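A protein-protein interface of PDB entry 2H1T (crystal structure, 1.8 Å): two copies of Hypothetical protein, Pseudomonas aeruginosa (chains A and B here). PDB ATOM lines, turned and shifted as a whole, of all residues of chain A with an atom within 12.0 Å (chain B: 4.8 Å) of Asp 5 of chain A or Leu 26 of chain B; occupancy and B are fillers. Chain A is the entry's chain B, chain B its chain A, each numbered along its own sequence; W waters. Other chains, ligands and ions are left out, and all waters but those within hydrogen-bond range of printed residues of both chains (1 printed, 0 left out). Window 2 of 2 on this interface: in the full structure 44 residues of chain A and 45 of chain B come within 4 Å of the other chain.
Asp 5 of chain A touches three residues of chain B.
Leu 26 of chain B touches three residues of chain A.
Of chain A, only Arg 6, Leu 7, Tyr 8 and Trp 10 come within 4 Å of Leu 24 of chain B.
Arg 25 of chain B touches just these residues of chain A: Asp 5 (3.5 Å), Arg 6 (3.5 Å) and Leu 7 (3.7 Å).
Of chain A, only Asp 5 (3.5 Å) comes within 4 Å of Glu 27 of chain B.
No residue of chain A comes within 4 Å of Ala 31 of chain B.
Of the printed residues of chain A, Leu 177 of chain B touches Tyr 8 (3.7 Å).
Printed residues of chain B within 4 Å of Trp 10 of chain A: Leu 24 (3.98 Å) and Phe 110 (3.9 Å).
Printed residues of chain B within 4 Å of Leu 7 of chain A: Leu 24 (3.4 Å) and Arg 25 (3.7 Å).
Printed residues of chain B within 4 Å of Tyr 8 of chain A: Leu 24 (2.7 Å), Leu 26 (3.8 Å) and Leu 177 (3.7 Å).
The nearest residue of chain A that does not touch Leu 26 of chain B is Leu 7 of chain A (5.1 Å).
The nearest printed residue of chain A that does not touch Leu 177 of chain B is Trp 10 of chain A (4.3 Å).
No position is printed for both chains.
Of the 13 pairs that touch across the chains among the printed residues, none has its exchanged pair printed and touching as well.
Among the printed residues, pairs that only touch across the chains: Leu 7 of chain A with Leu 24 of chain B, Asp 5 of chain A with Glu 27 of chain B, Arg 6 of chain A with Arg 25 of chain B, Asp 5 of chain A with Leu 26 of chain B, Leu 7 of chain A with Arg 25 of chain B, Tyr 8 of chain A with Leu 177 of chain B, Arg 6 of chain A with Leu 24 of chain B, Tyr 8 of chain A with Leu 26 of chain B, Trp 10 of chain A with Phe 110 of chain B and Trp 10 of chain A with Leu 24 of chain B.
Of the 6 printed residues of chain A, 5 touch a printed residue of chain B.
Printed residues of chain A that touch a printed residue of chain B: Asp 5, Arg 6, Leu 7, Tyr 8 and Trp 10.
Among the printed residues, 13 pairs touch across the chains.
Water W1 bridges the backbone carbonyl oxygen of Leu 24 of chain B (3.2 Å) and the backbone carbonyl oxygen of Tyr 8 of chain A (3.4 Å).
The guanidinium group of Arg 25 of chain B lies within salt-bridge range of the side-chain carboxylate of Asp 5 of chain A, at 3.5 Å.
The backbone NH (N) of Leu 24 of chain B is in hydrogen-bond range of the backbone carbonyl oxygen (O) of Tyr 8 of chain A (2.7 Å).
N of Leu 26 of chain B is in hydrogen-bond range of O of Arg 6 of chain A (2.8 Å).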
ATOM      1  N   ASP A   5       1.350   6.020 -16.996  1.00  0.00           N
ATOM      2  CA  ASP A   5       2.575   5.145 -16.854  1.00  0.00           C
ATOM      3  C   ASP A   5       2.306   3.899 -16.016  1.00  0.00           C
ATOM      4  O   ASP A   5       1.882   3.983 -14.860  1.00  0.00           O
ATOM      5  CB  ASP A   5       3.746   5.918 -16.239  1.00  0.00           C
ATOM      6  CG  ASP A   5       4.322   6.961 -17.187  1.00  0.00           C
ATOM      7  OD1 ASP A   5       3.627   7.344 -18.176  1.00  0.00           O
ATOM      8  OD2 ASP A   5       5.473   7.378 -16.939  1.00  0.00           O
ATOM      9  N   ARG A   6       2.597   2.750 -16.610  1.00  0.00           N
ATOM     10  CA  ARG A   6       2.320   1.463 -16.023  1.00  0.00           C
ATOM     11  C   ARG A   6       3.557   0.978 -15.257  1.00  0.00           C
ATOM     12  O   ARG A   6       4.701   1.118 -15.707  1.00  0.00           O
ATOM     13  CB  ARG A   6       1.950   0.472 -17.133  1.00  0.00           C
ATOM     14  CG  ARG A   6       0.618   0.769 -17.832  1.00  0.00           C
ATOM     15  CD  ARG A   6      -0.467  -0.232 -17.444  1.00  0.00           C
ATOM     16  N   LEU A   7       3.310   0.385 -14.099  1.00  0.00           N
ATOM     17  CA  LEU A   7       4.362  -0.130 -13.252  1.00  0.00           C
ATOM     18  C   LEU A   7       4.369  -1.637 -13.330  1.00  0.00           C
ATOM     19  O   LEU A   7       3.294  -2.262 -13.335  1.00  0.00           O
ATOM     20  CB  LEU A   7       4.146   0.303 -11.813  1.00  0.00           C
ATOM     21  CG  LEU A   7       4.168   1.806 -11.488  1.00  0.00           C
ATOM     22  CD1 LEU A   7       4.174   2.030  -9.967  1.00  0.00           C
ATOM     23  CD2 LEU A   7       5.353   2.532 -12.112  1.00  0.00           C
ATOM     24  N   TYR A   8       5.580  -2.203 -13.399  1.00  0.00           N
ATOM     25  CA  TYR A   8       5.784  -3.653 -13.520  1.00  0.00           C
ATOM     26  C   TYR A   8       6.871  -4.056 -12.538  1.00  0.00           C
ATOM     27  O   TYR A   8       7.904  -3.373 -12.416  1.00  0.00           O
ATOM     28  CB  TYR A   8       6.126  -4.047 -14.983  1.00  0.00           C
ATOM     29  CG  TYR A   8       5.036  -3.778 -15.991  1.00  0.00           C
ATOM     30  CD1 TYR A   8       4.934  -2.540 -16.630  1.00  0.00           C
ATOM     31  CD2 TYR A   8       4.090  -4.750 -16.302  1.00  0.00           C
ATOM     32  CE1 TYR A   8       3.953  -2.292 -17.553  1.00  0.00           C
ATOM     33  CE2 TYR A   8       3.070  -4.491 -17.245  1.00  0.00           C
ATOM     34  CZ  TYR A   8       3.015  -3.260 -17.869  1.00  0.00           C
ATOM     35  OH  TYR A   8       2.008  -2.978 -18.788  1.00  0.00           O
ATOM     36  N   THR A   9       6.595  -5.085 -11.737  1.00  0.00           N
ATOM     37  CA  THR A   9       7.580  -5.580 -10.760  1.00  0.00           C
ATOM     38  C   THR A   9       7.743  -7.061 -10.970  1.00  0.00           C
ATOM     39  O   THR A   9       6.747  -7.786 -11.081  1.00  0.00           O
ATOM     40  CB  THR A   9       7.147  -5.311  -9.272  1.00  0.00           C
ATOM     41  OG1 THR A   9       7.016  -3.907  -9.051  1.00  0.00           O
ATOM     42  CG2 THR A   9       8.164  -5.802  -8.305  1.00  0.00           C
ATOM     43  N   TRP A  10       8.990  -7.501 -11.071  1.00  0.00           N
ATOM     44  CA  TRP A  10       9.329  -8.922 -11.166  1.00  0.00           C
ATOM     45  C   TRP A  10      10.256  -9.322 -10.034  1.00  0.00           C
ATOM     46  O   TRP A  10      11.227  -8.627  -9.704  1.00  0.00           O
ATOM     47  CB  TRP A  10      10.014  -9.286 -12.492  1.00  0.00           C
ATOM     48  CG  TRP A  10       9.183  -9.049 -13.768  1.00  0.00           C
ATOM     49  CD1 TRP A  10       8.353  -9.924 -14.351  1.00  0.00           C
ATOM     50  CD2 TRP A  10       9.235  -7.898 -14.639  1.00  0.00           C
ATOM     51  NE1 TRP A  10       7.844  -9.407 -15.501  1.00  0.00           N
ATOM     52  CE2 TRP A  10       8.354  -8.153 -15.711  1.00  0.00           C
ATOM     53  CE3 TRP A  10       9.895  -6.643 -14.578  1.00  0.00           C
ATOM     54  CZ2 TRP A  10       8.127  -7.216 -16.764  1.00  0.00           C
ATOM     55  CZ3 TRP A  10       9.700  -5.726 -15.636  1.00  0.00           C
ATOM     56  CH2 TRP A  10       8.788  -6.024 -16.705  1.00  0.00           C
ATOM     57  N   LEU B  24       9.924  -1.538 -12.599  1.00  0.00           N
ATOM     58  CA  LEU B  24      10.038  -0.810 -13.846  1.00  0.00           C
ATOM     59  C   LEU B  24       8.820   0.099 -14.104  1.00  0.00           C
ATOM     60  O   LEU B  24       7.676  -0.275 -13.808  1.00  0.00           O
ATOM     61  CB  LEU B  24      10.220  -1.815 -14.980  1.00  0.00           C
ATOM     62  CG  LEU B  24      10.315  -1.334 -16.427  1.00  0.00           C
ATOM     63  CD1 LEU B  24      11.142  -2.371 -17.211  1.00  0.00           C
ATOM     64  CD2 LEU B  24       8.929  -1.168 -17.037  1.00  0.00           C
ATOM     65  N   ARG B  25       9.090   1.271 -14.677  1.00  0.00           N
ATOM     66  CA  ARG B  25       8.027   2.170 -15.148  1.00  0.00           C
ATOM     67  C   ARG B  25       8.043   2.200 -16.677  1.00  0.00           C
ATOM     68  O   ARG B  25       9.087   2.424 -17.284  1.00  0.00           O
ATOM     69  CB  ARG B  25       8.217   3.592 -14.631  1.00  0.00           C
ATOM     70  CG  ARG B  25       6.973   4.452 -14.804  1.00  0.00           C
ATOM     71  CD  ARG B  25       7.144   5.857 -14.229  1.00  0.00           C
ATOM     72  NE  ARG B  25       8.226   6.574 -14.906  1.00  0.00           N
ATOM     73  CZ  ARG B  25       9.440   6.784 -14.414  1.00  0.00           C
ATOM     74  NH1 ARG B  25       9.774   6.362 -13.193  1.00  0.00           N
ATOM     75  NH2 ARG B  25      10.334   7.443 -15.158  1.00  0.00           N
ATOM     76  N   LEU B  26       6.879   2.016 -17.281  1.00  0.00           N
ATOM     77  CA  LEU B  26       6.798   1.900 -18.715  1.00  0.00           C
ATOM     78  C   LEU B  26       5.982   3.045 -19.267  1.00  0.00           C
ATOM     79  O   LEU B  26       4.838   3.265 -18.865  1.00  0.00           O
ATOM     80  CB  LEU B  26       6.155   0.565 -19.122  1.00  0.00           C
ATOM     81  CG  LEU B  26       6.006   0.348 -20.637  1.00  0.00           C
ATOM     82  CD1 LEU B  26       7.397   0.326 -21.307  1.00  0.00           C
ATOM     83  CD2 LEU B  26       5.257  -0.938 -20.910  1.00  0.00           C
ATOM     84  N   GLU B  27       6.599   3.761 -20.207  1.00  0.00           N
ATOM     85  CA  GLU B  27       5.888   4.686 -21.105  1.00  0.00           C
ATOM     86  C   GLU B  27       5.764   4.095 -22.508  1.00  0.00           C
ATOM     87  O   GLU B  27       6.211   2.985 -22.775  1.00  0.00           O
ATOM     88  CB  GLU B  27       6.643   5.999 -21.175  1.00  0.00           C
ATOM     89  CG  GLU B  27       7.132   6.521 -19.853  1.00  0.00           C
ATOM     90  CD  GLU B  27       7.887   7.817 -20.023  1.00  0.00           C
ATOM     91  OE1 GLU B  27       7.563   8.582 -20.956  1.00  0.00           O
ATOM     92  OE2 GLU B  27       8.816   8.057 -19.232  1.00  0.00           O
ATOM     93  N   ASP B  28       5.166   4.840 -23.423  1.00  0.00           N
ATOM     94  CA  ASP B  28       4.920   4.332 -24.748  1.00  0.00           C
ATOM     95  C   ASP B  28       6.206   3.970 -25.483  1.00  0.00           C
ATOM     96  O   ASP B  28       6.264   2.935 -26.163  1.00  0.00           O
ATOM     97  CB  ASP B  28       4.116   5.347 -25.592  1.00  0.00           C
ATOM     98  CG  ASP B  28       2.649   5.468 -25.147  1.00  0.00           C
ATOM     99  OD1 ASP B  28       2.065   4.459 -24.684  1.00  0.00           O
ATOM    100  OD2 ASP B  28       2.092   6.594 -25.267  1.00  0.00           O
ATOM    101  N   GLN B  30       9.551   4.394 -24.004  1.00  0.00           N
ATOM    102  CA  GLN B  30      10.682   4.234 -23.104  1.00  0.00           C
ATOM    103  C   GLN B  30      10.312   3.590 -21.755  1.00  0.00           C
ATOM    104  O   GLN B  30       9.152   3.511 -21.369  1.00  0.00           O
ATOM    105  CB  GLN B  30      11.431   5.558 -22.912  1.00  0.00           C
ATOM    106  CG  GLN B  30      10.676   6.600 -22.162  1.00  0.00           C
ATOM    107  CD  GLN B  30      11.504   7.866 -22.031  1.00  0.00           C
ATOM    108  OE1 GLN B  30      11.628   8.632 -22.987  1.00  0.00           O
ATOM    109  NE2 GLN B  30      12.086   8.074 -20.863  1.00  0.00           N
ATOM    110  N   ALA B  31      11.321   3.037 -21.101  1.00  0.00           N
ATOM    111  CA  ALA B  31      11.169   2.464 -19.777  1.00  0.00           C
ATOM    112  C   ALA B  31      12.327   2.894 -18.934  1.00  0.00           C
ATOM    113  O   ALA B  31      13.433   3.153 -19.432  1.00  0.00           O
ATOM    114  CB  ALA B  31      11.082   0.931 -19.800  1.00  0.00           C
ATOM    115  N   TRP B  54      12.954   3.276 -27.451  1.00  0.00           N
ATOM    116  CA  TRP B  54      12.799   2.563 -28.745  1.00  0.00           C
ATOM    117  C   TRP B  54      11.928   3.364 -29.677  1.00  0.00           C
ATOM    118  O   TRP B  54      11.355   4.369 -29.251  1.00  0.00           O
ATOM    119  CB  TRP B  54      12.195   1.185 -28.519  1.00  0.00           C
ATOM    120  CG  TRP B  54      10.964   1.175 -27.706  1.00  0.00           C
ATOM    121  CD1 TRP B  54       9.687   1.224 -28.164  1.00  0.00           C
ATOM    122  CD2 TRP B  54      10.881   1.111 -26.269  1.00  0.00           C
ATOM    123  NE1 TRP B  54       8.807   1.189 -27.113  1.00  0.00           N
ATOM    124  CE2 TRP B  54       9.509   1.088 -25.941  1.00  0.00           C
ATOM    125  CE3 TRP B  54      11.832   0.970 -25.234  1.00  0.00           C
ATOM    126  CZ2 TRP B  54       9.054   1.000 -24.623  1.00  0.00           C
ATOM    127  CZ3 TRP B  54      11.375   0.859 -23.915  1.00  0.00           C
ATOM    128  CH2 TRP B  54       9.996   0.912 -23.620  1.00  0.00           C
ATOM    129  N   PHE B 110      12.056  -8.213 -18.626  1.00  0.00           N
ATOM    130  CA  PHE B 110      11.525  -7.101 -19.452  1.00  0.00           C
ATOM    131  C   PHE B 110      11.915  -7.240 -20.906  1.00  0.00           C
ATOM    132  O   PHE B 110      11.062  -7.097 -21.805  1.00  0.00           O
ATOM    133  CB  PHE B 110      11.958  -5.727 -18.968  1.00  0.00           C
ATOM    134  CG  PHE B 110      11.490  -4.596 -19.862  1.00  0.00           C
ATOM    135  CD1 PHE B 110      10.137  -4.485 -20.245  1.00  0.00           C
ATOM    136  CD2 PHE B 110      12.357  -3.653 -20.294  1.00  0.00           C
ATOM    137  CE1 PHE B 110       9.691  -3.463 -21.064  1.00  0.00           C
ATOM    138  CE2 PHE B 110      11.908  -2.625 -21.123  1.00  0.00           C
ATOM    139  CZ  PHE B 110      10.586  -2.533 -21.506  1.00  0.00           C
ATOM    140  N   LEU B 177       4.335  -8.163 -22.197  1.00  0.00           N
ATOM    141  CA  LEU B 177       5.090  -8.184 -20.965  1.00  0.00           C
ATOM    142  C   LEU B 177       5.007  -9.564 -20.309  1.00  0.00           C
ATOM    143  O   LEU B 177       3.940 -10.135 -20.159  1.00  0.00           O
ATOM    144  CB  LEU B 177       4.652  -7.081 -19.990  1.00  0.00           C
ATOM    145  CG  LEU B 177       4.928  -5.609 -20.272  1.00  0.00           C
ATOM    146  CD1 LEU B 177       6.457  -5.314 -20.272  1.00  0.00           C
ATOM    147  CD2 LEU B 177       4.257  -5.083 -21.513  1.00  0.00           C
HETATM  148  O   HOH W   1       7.432  -0.569 -10.631  1.00  0.00           O
